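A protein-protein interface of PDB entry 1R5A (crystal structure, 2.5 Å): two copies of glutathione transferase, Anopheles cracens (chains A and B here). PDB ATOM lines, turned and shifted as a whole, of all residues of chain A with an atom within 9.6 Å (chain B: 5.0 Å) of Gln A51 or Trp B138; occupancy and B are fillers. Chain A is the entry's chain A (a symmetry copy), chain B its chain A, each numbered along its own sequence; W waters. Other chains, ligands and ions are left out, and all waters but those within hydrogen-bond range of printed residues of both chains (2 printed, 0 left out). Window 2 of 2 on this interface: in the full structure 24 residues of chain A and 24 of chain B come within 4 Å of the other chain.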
ATOM      1  N   LEU A  33     -30.540  15.328 -26.146  1.00  0.00           N
ATOM      2  CA  LEU A  33     -30.417  14.096 -26.901  1.00  0.00           C
ATOM      3  C   LEU A  33     -31.630  13.247 -26.574  1.00  0.00           C
ATOM      4  O   LEU A  33     -31.683  12.605 -25.525  1.00  0.00           O
ATOM      5  CB  LEU A  33     -29.125  13.379 -26.503  1.00  0.00           C
ATOM      6  CG  LEU A  33     -28.336  12.698 -27.625  1.00  0.00           C
ATOM      7  CD1 LEU A  33     -28.159  13.652 -28.801  1.00  0.00           C
ATOM      8  CD2 LEU A  33     -26.982  12.251 -27.084  1.00  0.00           C
ATOM      9  N   ILE A  35     -33.197  10.385 -26.280  1.00  0.00           N
ATOM     10  CA  ILE A  35     -32.884   8.971 -26.247  1.00  0.00           C
ATOM     11  C   ILE A  35     -34.093   8.126 -26.594  1.00  0.00           C
ATOM     12  O   ILE A  35     -33.973   7.013 -27.120  1.00  0.00           O
ATOM     13  CB  ILE A  35     -32.339   8.630 -24.869  1.00  0.00           C
ATOM     14  CG1 ILE A  35     -31.004   9.362 -24.720  1.00  0.00           C
ATOM     15  CG2 ILE A  35     -32.229   7.121 -24.679  1.00  0.00           C
ATOM     16  CD1 ILE A  35     -30.322   9.134 -23.440  1.00  0.00           C
ATOM     17  N   GLN A  40     -29.257   9.239 -29.688  1.00  0.00           N
ATOM     18  CA  GLN A  40     -27.920   8.889 -29.236  1.00  0.00           C
ATOM     19  C   GLN A  40     -27.288   7.784 -30.080  1.00  0.00           C
ATOM     20  O   GLN A  40     -26.072   7.576 -30.025  1.00  0.00           O
ATOM     21  CB  GLN A  40     -27.944   8.453 -27.773  1.00  0.00           C
ATOM     22  CG  GLN A  40     -28.328   7.003 -27.527  1.00  0.00           C
ATOM     23  CD  GLN A  40     -29.812   6.728 -27.684  1.00  0.00           C
ATOM     24  OE1 GLN A  40     -30.359   5.861 -27.003  1.00  0.00           O
ATOM     25  NE2 GLN A  40     -30.464   7.445 -28.587  1.00  0.00           N
ATOM     26  N   LEU A  41     -28.107   7.083 -30.864  1.00  0.00           N
ATOM     27  CA  LEU A  41     -27.608   5.998 -31.698  1.00  0.00           C
ATOM     28  C   LEU A  41     -27.017   6.451 -33.025  1.00  0.00           C
ATOM     29  O   LEU A  41     -26.409   5.654 -33.743  1.00  0.00           O
ATOM     30  CB  LEU A  41     -28.702   4.965 -31.943  1.00  0.00           C
ATOM     31  CG  LEU A  41     -29.359   4.356 -30.694  1.00  0.00           C
ATOM     32  CD1 LEU A  41     -30.149   3.130 -31.117  1.00  0.00           C
ATOM     33  CD2 LEU A  41     -28.318   3.966 -29.654  1.00  0.00           C
ATOM     34  N   LYS A  42     -27.171   7.730 -33.353  1.00  0.00           N
ATOM     35  CA  LYS A  42     -26.602   8.227 -34.605  1.00  0.00           C
ATOM     36  C   LYS A  42     -25.069   8.141 -34.619  1.00  0.00           C
ATOM     37  O   LYS A  42     -24.400   8.375 -33.606  1.00  0.00           O
ATOM     38  CB  LYS A  42     -27.063   9.654 -34.874  1.00  0.00           C
ATOM     39  CG  LYS A  42     -28.524   9.711 -35.264  1.00  0.00           C
ATOM     40  CD  LYS A  42     -29.051  11.123 -35.312  1.00  0.00           C
ATOM     41  CE  LYS A  42     -30.570  11.097 -35.284  1.00  0.00           C
ATOM     42  NZ  LYS A  42     -31.181  12.439 -35.530  1.00  0.00           N
ATOM     43  N   PHE A  45     -22.571  10.551 -32.803  1.00  0.00           N
ATOM     44  CA  PHE A  45     -22.528  10.601 -31.344  1.00  0.00           C
ATOM     45  C   PHE A  45     -21.832   9.332 -30.895  1.00  0.00           C
ATOM     46  O   PHE A  45     -20.992   9.359 -29.988  1.00  0.00           O
ATOM     47  CB  PHE A  45     -23.923  10.655 -30.707  1.00  0.00           C
ATOM     48  CG  PHE A  45     -23.892  10.804 -29.193  1.00  0.00           C
ATOM     49  CD1 PHE A  45     -23.360  11.951 -28.600  1.00  0.00           C
ATOM     50  CD2 PHE A  45     -24.359   9.783 -28.363  1.00  0.00           C
ATOM     51  CE1 PHE A  45     -23.291  12.070 -27.211  1.00  0.00           C
ATOM     52  CE2 PHE A  45     -24.293   9.897 -26.967  1.00  0.00           C
ATOM     53  CZ  PHE A  45     -23.759  11.038 -26.397  1.00  0.00           C
ATOM     54  N   VAL A  46     -22.178   8.220 -31.546  1.00  0.00           N
ATOM     55  CA  VAL A  46     -21.586   6.927 -31.234  1.00  0.00           C
ATOM     56  C   VAL A  46     -20.093   6.978 -31.530  1.00  0.00           C
ATOM     57  O   VAL A  46     -19.308   6.198 -30.985  1.00  0.00           O
ATOM     58  CB  VAL A  46     -22.221   5.800 -32.070  1.00  0.00           C
ATOM     59  CG1 VAL A  46     -21.624   4.460 -31.669  1.00  0.00           C
ATOM     60  CG2 VAL A  46     -23.729   5.789 -31.871  1.00  0.00           C
ATOM     61  N   GLU A  47     -19.701   7.897 -32.404  1.00  0.00           N
ATOM     62  CA  GLU A  47     -18.297   8.047 -32.743  1.00  0.00           C
ATOM     63  C   GLU A  47     -17.681   8.859 -31.628  1.00  0.00           C
ATOM     64  O   GLU A  47     -16.491   8.731 -31.324  1.00  0.00           O
ATOM     65  CB  GLU A  47     -18.143   8.783 -34.076  1.00  0.00           C
ATOM     66  CG  GLU A  47     -17.968   7.870 -35.285  1.00  0.00           C
ATOM     67  CD  GLU A  47     -18.379   8.547 -36.588  1.00  0.00           C
ATOM     68  OE1 GLU A  47     -18.079   9.752 -36.765  1.00  0.00           O
ATOM     69  OE2 GLU A  47     -19.000   7.869 -37.439  1.00  0.00           O
ATOM     70  N   LEU A  48     -18.515   9.689 -31.012  1.00  0.00           N
ATOM     71  CA  LEU A  48     -18.071  10.544 -29.917  1.00  0.00           C
ATOM     72  C   LEU A  48     -17.936   9.718 -28.638  1.00  0.00           C
ATOM     73  O   LEU A  48     -16.906   9.760 -27.962  1.00  0.00           O
ATOM     74  CB  LEU A  48     -19.076  11.686 -29.689  1.00  0.00           C
ATOM     75  CG  LEU A  48     -18.615  12.805 -28.749  1.00  0.00           C
ATOM     76  CD1 LEU A  48     -17.443  13.524 -29.376  1.00  0.00           C
ATOM     77  CD2 LEU A  48     -19.750  13.786 -28.489  1.00  0.00           C
ATOM     78  N   ASN A  49     -18.979   8.948 -28.345  1.00  0.00           N
ATOM     79  CA  ASN A  49     -19.042   8.113 -27.155  1.00  0.00           C
ATOM     80  C   ASN A  49     -19.492   6.698 -27.539  1.00  0.00           C
ATOM     81  O   ASN A  49     -20.667   6.465 -27.839  1.00  0.00           O
ATOM     82  CB  ASN A  49     -20.027   8.750 -26.178  1.00  0.00           C
ATOM     83  CG  ASN A  49     -20.231   7.930 -24.941  1.00  0.00           C
ATOM     84  OD1 ASN A  49     -20.996   8.314 -24.056  1.00  0.00           O
ATOM     85  ND2 ASN A  49     -19.554   6.794 -24.861  1.00  0.00           N
ATOM     86  N   PRO A  50     -18.557   5.728 -27.524  1.00  0.00           N
ATOM     87  CA  PRO A  50     -18.861   4.339 -27.877  1.00  0.00           C
ATOM     88  C   PRO A  50     -20.133   3.820 -27.205  1.00  0.00           C
ATOM     89  O   PRO A  50     -21.018   3.265 -27.863  1.00  0.00           O
ATOM     90  CB  PRO A  50     -17.611   3.583 -27.415  1.00  0.00           C
ATOM     91  CG  PRO A  50     -16.525   4.590 -27.554  1.00  0.00           C
ATOM     92  CD  PRO A  50     -17.169   5.853 -27.040  1.00  0.00           C
ATOM     93  N   GLN A  51     -20.211   3.998 -25.892  1.00  0.00           N
ATOM     94  CA  GLN A  51     -21.355   3.556 -25.113  1.00  0.00           C
ATOM     95  C   GLN A  51     -22.609   4.419 -25.387  1.00  0.00           C
ATOM     96  O   GLN A  51     -23.667   4.190 -24.813  1.00  0.00           O
ATOM     97  CB  GLN A  51     -20.973   3.579 -23.622  1.00  0.00           C
ATOM     98  CG  GLN A  51     -22.007   2.987 -22.668  1.00  0.00           C
ATOM     99  CD  GLN A  51     -21.434   2.651 -21.285  1.00  0.00           C
ATOM    100  OE1 GLN A  51     -22.182   2.285 -20.375  1.00  0.00           O
ATOM    101  NE2 GLN A  51     -20.108   2.760 -21.128  1.00  0.00           N
ATOM    102  N   HIS A  52     -22.485   5.400 -26.276  1.00  0.00           N
ATOM    103  CA  HIS A  52     -23.589   6.294 -26.644  1.00  0.00           C
ATOM    104  C   HIS A  52     -24.625   6.597 -25.544  1.00  0.00           C
ATOM    105  O   HIS A  52     -25.818   6.313 -25.693  1.00  0.00           O
ATOM    106  CB  HIS A  52     -24.300   5.762 -27.911  1.00  0.00           C
ATOM    107  CG  HIS A  52     -24.879   4.385 -27.764  1.00  0.00           C
ATOM    108  ND1 HIS A  52     -26.012   4.124 -27.026  1.00  0.00           N
ATOM    109  CD2 HIS A  52     -24.462   3.189 -28.244  1.00  0.00           C
ATOM    110  CE1 HIS A  52     -26.267   2.829 -27.051  1.00  0.00           C
ATOM    111  NE2 HIS A  52     -25.342   2.238 -27.783  1.00  0.00           N
ATOM    112  N   CYS A  53     -24.171   7.201 -24.449  1.00  0.00           N
ATOM    113  CA  CYS A  53     -25.064   7.538 -23.346  1.00  0.00           C
ATOM    114  C   CYS A  53     -24.911   8.983 -22.895  1.00  0.00           C
ATOM    115  O   CYS A  53     -23.960   9.676 -23.265  1.00  0.00           O
ATOM    116  CB  CYS A  53     -24.798   6.615 -22.156  1.00  0.00           C
ATOM    117  SG  CYS A  53     -23.083   6.672 -21.530  1.00  0.00           S
ATOM    118  N   ILE A  54     -25.856   9.429 -22.081  1.00  0.00           N
ATOM    119  CA  ILE A  54     -25.814  10.775 -21.546  1.00  0.00           C
ATOM    120  C   ILE A  54     -25.952  10.699 -20.028  1.00  0.00           C
ATOM    121  O   ILE A  54     -26.611   9.802 -19.497  1.00  0.00           O
ATOM    122  CB  ILE A  54     -26.937  11.638 -22.115  1.00  0.00           C
ATOM    123  CG1 ILE A  54     -28.297  11.004 -21.787  1.00  0.00           C
ATOM    124  CG2 ILE A  54     -26.726  11.804 -23.601  1.00  0.00           C
ATOM    125  CD1 ILE A  54     -29.489  11.854 -22.173  1.00  0.00           C
ATOM    126  N   PRO A  55     -25.381  11.681 -19.312  1.00  0.00           N
ATOM    127  CA  PRO A  55     -24.655  12.810 -19.893  1.00  0.00           C
ATOM    128  C   PRO A  55     -23.299  12.516 -20.517  1.00  0.00           C
ATOM    129  O   PRO A  55     -22.576  11.611 -20.087  1.00  0.00           O
ATOM    130  CB  PRO A  55     -24.535  13.764 -18.717  1.00  0.00           C
ATOM    131  CG  PRO A  55     -24.286  12.820 -17.577  1.00  0.00           C
ATOM    132  CD  PRO A  55     -25.307  11.717 -17.836  1.00  0.00           C
ATOM    133  N   THR A  56     -22.980  13.293 -21.557  1.00  0.00           N
ATOM    134  CA  THR A  56     -21.694  13.223 -22.232  1.00  0.00           C
ATOM    135  C   THR A  56     -21.168  14.661 -22.340  1.00  0.00           C
ATOM    136  O   THR A  56     -21.839  15.558 -22.853  1.00  0.00           O
ATOM    137  CB  THR A  56     -21.794  12.579 -23.635  1.00  0.00           C
ATOM    138  OG1 THR A  56     -21.932  11.158 -23.496  1.00  0.00           O
ATOM    139  CG2 THR A  56     -20.543  12.863 -24.441  1.00  0.00           C
ATOM    140  N   VAL A  63     -13.556  14.926 -24.219  1.00  0.00           N
ATOM    141  CA  VAL A  63     -14.797  14.173 -24.166  1.00  0.00           C
ATOM    142  C   VAL A  63     -14.750  13.314 -22.911  1.00  0.00           C
ATOM    143  O   VAL A  63     -13.688  12.824 -22.529  1.00  0.00           O
ATOM    144  CB  VAL A  63     -14.959  13.271 -25.410  1.00  0.00           C
ATOM    145  CG1 VAL A  63     -16.274  12.497 -25.332  1.00  0.00           C
ATOM    146  CG2 VAL A  63     -14.919  14.128 -26.667  1.00  0.00           C
ATOM    147  N   TRP A  65     -17.724  10.876 -20.180  1.00  0.00           N
ATOM    148  CA  TRP A  65     -19.091  10.519 -19.800  1.00  0.00           C
ATOM    149  C   TRP A  65     -19.087   9.797 -18.445  1.00  0.00           C
ATOM    150  O   TRP A  65     -18.034   9.383 -17.961  1.00  0.00           O
ATOM    151  CB  TRP A  65     -19.804   9.692 -20.915  1.00  0.00           C
ATOM    152  CG  TRP A  65     -19.193   8.361 -21.296  1.00  0.00           C
ATOM    153  CD1 TRP A  65     -19.517   7.134 -20.786  1.00  0.00           C
ATOM    154  CD2 TRP A  65     -18.149   8.131 -22.262  1.00  0.00           C
ATOM    155  NE1 TRP A  65     -18.742   6.157 -21.368  1.00  0.00           N
ATOM    156  CE2 TRP A  65     -17.894   6.739 -22.274  1.00  0.00           C
ATOM    157  CE3 TRP A  65     -17.409   8.965 -23.111  1.00  0.00           C
ATOM    158  CZ2 TRP A  65     -16.923   6.160 -23.108  1.00  0.00           C
ATOM    159  CZ3 TRP A  65     -16.441   8.391 -23.942  1.00  0.00           C
ATOM    160  CH2 TRP A  65     -16.209   6.997 -23.931  1.00  0.00           C
ATOM    161  N   GLU A  66     -20.271   9.677 -17.848  1.00  0.00           N
ATOM    162  CA  GLU A  66     -20.504   9.069 -16.527  1.00  0.00           C
ATOM    163  C   GLU A  66     -20.701  10.236 -15.585  1.00  0.00           C
ATOM    164  O   GLU A  66     -19.744  10.826 -15.102  1.00  0.00           O
ATOM    165  CB  GLU A  66     -19.322   8.226 -16.063  1.00  0.00           C
ATOM    166  CG  GLU A  66     -19.334   6.827 -16.605  1.00  0.00           C
ATOM    167  CD  GLU A  66     -20.513   6.016 -16.090  1.00  0.00           C
ATOM    168  OE1 GLU A  66     -21.096   6.398 -15.053  1.00  0.00           O
ATOM    169  OE2 GLU A  66     -20.849   4.985 -16.713  1.00  0.00           O
ATOM    170  N   LEU A 103     -23.659   4.807  -7.632  1.00  0.00           N
ATOM    171  CA  LEU A 103     -23.642   4.228  -8.958  1.00  0.00           C
ATOM    172  C   LEU A 103     -23.872   2.720  -8.954  1.00  0.00           C
ATOM    173  O   LEU A 103     -24.769   2.217  -9.649  1.00  0.00           O
ATOM    174  CB  LEU A 103     -22.323   4.532  -9.668  1.00  0.00           C
ATOM    175  CG  LEU A 103     -22.130   3.831 -11.027  1.00  0.00           C
ATOM    176  CD1 LEU A 103     -23.303   4.149 -11.936  1.00  0.00           C
ATOM    177  CD2 LEU A 103     -20.823   4.276 -11.676  1.00  0.00           C
ATOM    178  N   GLN A 108     -28.540   2.003  -8.942  1.00  0.00           N
ATOM    179  CA  GLN A 108     -28.681   0.804  -9.753  1.00  0.00           C
ATOM    180  C   GLN A 108     -29.982   0.103  -9.385  1.00  0.00           C
ATOM    181  O   GLN A 108     -30.757  -0.291 -10.262  1.00  0.00           O
ATOM    182  CB  GLN A 108     -27.490  -0.131  -9.525  1.00  0.00           C
ATOM    183  CG  GLN A 108     -27.440  -1.306 -10.484  1.00  0.00           C
ATOM    184  CD  GLN A 108     -27.181  -0.875 -11.926  1.00  0.00           C
ATOM    185  OE1 GLN A 108     -26.057  -0.484 -12.292  1.00  0.00           O
ATOM    186  NE2 GLN A 108     -28.223  -0.940 -12.756  1.00  0.00           N
ATOM    187  N   PHE B 101     -16.890   2.713 -15.612  1.00  0.00           N
ATOM    188  CA  PHE B 101     -17.345   1.858 -16.706  1.00  0.00           C
ATOM    189  C   PHE B 101     -17.368   0.416 -16.200  1.00  0.00           C
ATOM    190  O   PHE B 101     -18.349  -0.310 -16.357  1.00  0.00           O
ATOM    191  CB  PHE B 101     -16.369   1.975 -17.888  1.00  0.00           C
ATOM    192  CG  PHE B 101     -16.495   0.877 -18.903  1.00  0.00           C
ATOM    193  CD1 PHE B 101     -17.657   0.734 -19.660  1.00  0.00           C
ATOM    194  CD2 PHE B 101     -15.434  -0.003 -19.126  1.00  0.00           C
ATOM    195  CE1 PHE B 101     -17.763  -0.268 -20.632  1.00  0.00           C
ATOM    196  CE2 PHE B 101     -15.525  -1.011 -20.100  1.00  0.00           C
ATOM    197  CZ  PHE B 101     -16.697  -1.139 -20.853  1.00  0.00           C
ATOM    198  N   THR B 105     -20.768  -1.038 -15.507  1.00  0.00           N
ATOM    199  CA  THR B 105     -21.105  -1.650 -16.780  1.00  0.00           C
ATOM    200  C   THR B 105     -20.476  -3.004 -17.050  1.00  0.00           C
ATOM    201  O   THR B 105     -21.148  -4.025 -16.958  1.00  0.00           O
ATOM    202  CB  THR B 105     -20.779  -0.696 -17.968  1.00  0.00           C
ATOM    203  OG1 THR B 105     -21.348   0.589 -17.705  1.00  0.00           O
ATOM    204  CG2 THR B 105     -21.376  -1.212 -19.270  1.00  0.00           C
ATOM    205  N   ARG B 109     -22.282  -6.517 -15.648  1.00  0.00           N
ATOM    206  CA  ARG B 109     -22.813  -7.456 -16.634  1.00  0.00           C
ATOM    207  C   ARG B 109     -22.150  -8.835 -16.575  1.00  0.00           C
ATOM    208  O   ARG B 109     -22.695  -9.807 -17.099  1.00  0.00           O
ATOM    209  CB  ARG B 109     -22.679  -6.874 -18.045  1.00  0.00           C
ATOM    210  CG  ARG B 109     -23.641  -5.751 -18.301  1.00  0.00           C
ATOM    211  CD  ARG B 109     -23.485  -5.151 -19.672  1.00  0.00           C
ATOM    212  NE  ARG B 109     -24.292  -3.943 -19.786  1.00  0.00           N
ATOM    213  CZ  ARG B 109     -24.669  -3.391 -20.934  1.00  0.00           C
ATOM    214  NH1 ARG B 109     -24.314  -3.936 -22.090  1.00  0.00           N
ATOM    215  NH2 ARG B 109     -25.406  -2.288 -20.920  1.00  0.00           N
ATOM    216  N   GLU B 134     -21.911  -6.857 -25.731  1.00  0.00           N
ATOM    217  CA  GLU B 134     -22.097  -5.467 -26.120  1.00  0.00           C
ATOM    218  C   GLU B 134     -21.146  -4.536 -25.360  1.00  0.00           C
ATOM    219  O   GLU B 134     -20.616  -3.579 -25.928  1.00  0.00           O
ATOM    220  CB  GLU B 134     -23.541  -5.033 -25.857  1.00  0.00           C
ATOM    221  CG  GLU B 134     -23.742  -3.559 -26.109  1.00  0.00           C
ATOM    222  CD  GLU B 134     -25.162  -3.110 -25.903  1.00  0.00           C
ATOM    223  OE1 GLU B 134     -25.695  -3.256 -24.783  1.00  0.00           O
ATOM    224  OE2 GLU B 134     -25.740  -2.598 -26.876  1.00  0.00           O
ATOM    225  N   ALA B 135     -20.939  -4.812 -24.073  1.00  0.00           N
ATOM    226  CA  ALA B 135     -20.057  -3.997 -23.259  1.00  0.00           C
ATOM    227  C   ALA B 135     -18.617  -4.233 -23.681  1.00  0.00           C
ATOM    228  O   ALA B 135     -17.843  -3.278 -23.786  1.00  0.00           O
ATOM    229  CB  ALA B 135     -20.245  -4.319 -21.786  1.00  0.00           C
ATOM    230  N   LEU B 136     -18.246  -5.490 -23.924  1.00  0.00           N
ATOM    231  CA  LEU B 136     -16.876  -5.780 -24.359  1.00  0.00           C
ATOM    232  C   LEU B 136     -16.630  -4.996 -25.638  1.00  0.00           C
ATOM    233  O   LEU B 136     -15.514  -4.531 -25.896  1.00  0.00           O
ATOM    234  CB  LEU B 136     -16.683  -7.272 -24.626  1.00  0.00           C
ATOM    235  CG  LEU B 136     -16.420  -8.174 -23.414  1.00  0.00           C
ATOM    236  CD1 LEU B 136     -16.654  -9.626 -23.807  1.00  0.00           C
ATOM    237  CD2 LEU B 136     -14.986  -7.979 -22.904  1.00  0.00           C
ATOM    238  N   GLY B 137     -17.695  -4.852 -26.428  1.00  0.00           N
ATOM    239  CA  GLY B 137     -17.621  -4.111 -27.671  1.00  0.00           C
ATOM    240  C   GLY B 137     -17.293  -2.656 -27.389  1.00  0.00           C
ATOM    241  O   GLY B 137     -16.447  -2.074 -28.068  1.00  0.00           O
ATOM    242  N   TRP B 138     -17.955  -2.064 -26.393  1.00  0.00           N
ATOM    243  CA  TRP B 138     -17.694  -0.675 -26.032  1.00  0.00           C
ATOM    244  C   TRP B 138     -16.240  -0.559 -25.597  1.00  0.00           C
ATOM    245  O   TRP B 138     -15.513   0.336 -26.042  1.00  0.00           O
ATOM    246  CB  TRP B 138     -18.607  -0.224 -24.890  1.00  0.00           C
ATOM    247  CG  TRP B 138     -20.059  -0.165 -25.253  1.00  0.00           C
ATOM    248  CD1 TRP B 138     -20.585   0.066 -26.492  1.00  0.00           C
ATOM    249  CD2 TRP B 138     -21.175  -0.322 -24.368  1.00  0.00           C
ATOM    250  NE1 TRP B 138     -21.960   0.058 -26.437  1.00  0.00           N
ATOM    251  CE2 TRP B 138     -22.351  -0.177 -25.144  1.00  0.00           C
ATOM    252  CE3 TRP B 138     -21.301  -0.571 -22.994  1.00  0.00           C
ATOM    253  CZ2 TRP B 138     -23.633  -0.276 -24.594  1.00  0.00           C
ATOM    254  CZ3 TRP B 138     -22.571  -0.669 -22.451  1.00  0.00           C
ATOM    255  CH2 TRP B 138     -23.722  -0.522 -23.250  1.00  0.00           C
ATOM    256  N   PHE B 139     -15.819  -1.471 -24.722  1.00  0.00           N
ATOM    257  CA  PHE B 139     -14.439  -1.482 -24.247  1.00  0.00           C
ATOM    258  C   PHE B 139     -13.521  -1.566 -25.465  1.00  0.00           C
ATOM    259  O   PHE B 139     -12.557  -0.814 -25.575  1.00  0.00           O
ATOM    260  CB  PHE B 139     -14.207  -2.682 -23.317  1.00  0.00           C
ATOM    261  CG  PHE B 139     -12.859  -2.692 -22.633  1.00  0.00           C
ATOM    262  CD1 PHE B 139     -12.187  -1.500 -22.353  1.00  0.00           C
ATOM    263  CD2 PHE B 139     -12.289  -3.894 -22.222  1.00  0.00           C
ATOM    264  CE1 PHE B 139     -10.961  -1.504 -21.670  1.00  0.00           C
ATOM    265  CE2 PHE B 139     -11.065  -3.915 -21.539  1.00  0.00           C
ATOM    266  CZ  PHE B 139     -10.397  -2.717 -21.260  1.00  0.00           C
ATOM    267  N   GLU B 140     -13.829  -2.472 -26.390  1.00  0.00           N
ATOM    268  CA  GLU B 140     -13.005  -2.617 -27.589  1.00  0.00           C
ATOM    269  C   GLU B 140     -12.823  -1.263 -28.264  1.00  0.00           C
ATOM    270  O   GLU B 140     -11.723  -0.911 -28.684  1.00  0.00           O
ATOM    271  CB  GLU B 140     -13.647  -3.596 -28.563  1.00  0.00           C
ATOM    272  CG  GLU B 140     -12.830  -3.871 -29.821  1.00  0.00           C
ATOM    273  CD  GLU B 140     -11.535  -4.615 -29.545  1.00  0.00           C
ATOM    274  OE1 GLU B 140     -11.347  -5.100 -28.412  1.00  0.00           O
ATOM    275  OE2 GLU B 140     -10.700  -4.725 -30.472  1.00  0.00           O
ATOM    276  N   ALA B 141     -13.905  -0.499 -28.366  1.00  0.00           N
ATOM    277  CA  ALA B 141     -13.828   0.818 -28.984  1.00  0.00           C
ATOM    278  C   ALA B 141     -13.010   1.741 -28.091  1.00  0.00           C
ATOM    279  O   ALA B 141     -12.266   2.580 -28.578  1.00  0.00           O
ATOM    280  CB  ALA B 141     -15.234   1.395 -29.206  1.00  0.00           C
ATOM    281  N   MET B 142     -13.136   1.578 -26.779  1.00  0.00           N
ATOM    282  CA  MET B 142     -12.385   2.410 -25.836  1.00  0.00           C
ATOM    283  C   MET B 142     -10.874   2.159 -25.853  1.00  0.00           C
ATOM    284  O   MET B 142     -10.095   3.026 -25.483  1.00  0.00           O
ATOM    285  CB  MET B 142     -12.933   2.219 -24.419  1.00  0.00           C
ATOM    286  CG  MET B 142     -14.251   2.954 -24.178  1.00  0.00           C
ATOM    287  SD  MET B 142     -15.332   2.104 -23.022  1.00  0.00           S
ATOM    288  CE  MET B 142     -14.440   2.392 -21.466  1.00  0.00           C
HETATM  289  O   HOH W   1     -24.482  -0.159 -28.414  1.00  0.00           O
HETATM  290  O   HOH W   2     -21.250   2.245 -15.772  1.00  0.00           O
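OG1 of Thr B105 is in hydrogen-bond range of OE1 of Gln A51 (3.3 Å).
The backbone carbonyl oxygen of Phe B101 lies close to the side-chain hydroxyl of Thr B105, at 3.4 Å. The side-chain amide nitrogen (ND2) of Asn A49 sits close to the backbone NH (N) of Gln A51 (3.1 Å).
Pro A50 touches Trp B138. Ala B141 touches Pro A50 (CB to CB, 3.7 Å). Gln A51 touches Phe B101 (NE2 to CD1, 3.5 Å). Gln A51 touches Trp B138.
Gln A51 touches three residues of chain B. Trp B138 touches just these residues of chain A: Pro A50 and Gln A51. No residue of chain A comes within 4 Å of Gly B137. Ala B141 touches just one residue of chain A: Pro A50. Printed residues of chain A within 4 Å of Phe B101: Gln A51 (3.5 Å). Printed residues of chain A within 4 Å of Thr B105: Gln A51 (3.3 Å). Leu A33 touches none of the printed residues of chain B. Glu B140 touches none of the printed residues of chain A. The nearest residue of chain A that does not touch Trp B138 is His A52 (4.2 Å).
Of the 22 printed residues of chain A, 2 touch a printed residue of chain B. Hydrophobic or aromatic side chains of chain A that line the printed part of chain B: Pro A50. Along chain A the printed residues that touch a printed residue of chain B span positions 50 to 51. Of the 12 printed residues of chain B, 4 touch a printed residue of chain A. Printed residues of chain B that touch a printed residue of chain A: Phe B101, Thr B105, Trp B138 and Ala B141. Among the printed residues, 5 pairs touch across the chains. Among the printed residues, no Asp or Glu carboxylate lies within 4 Å of a Lys or Arg side-chain nitrogen of the other chain.
No position is printed for both chains. Of the 5 pairs that touch across the chains among the printed residues, none has its exchanged pair printed and touching as well.
Water W2 lies within hydrogen-bond range of OG1 of Thr B105 (2.5 Å) and OE2 of Glu A66 (2.9 Å). Water W1 lies within hydrogen-bond range of NE2 of His A52 (2.6 Å), OE2 of Glu B134 (3.1 Å) and NE1 of Trp B138 (3.2 Å).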
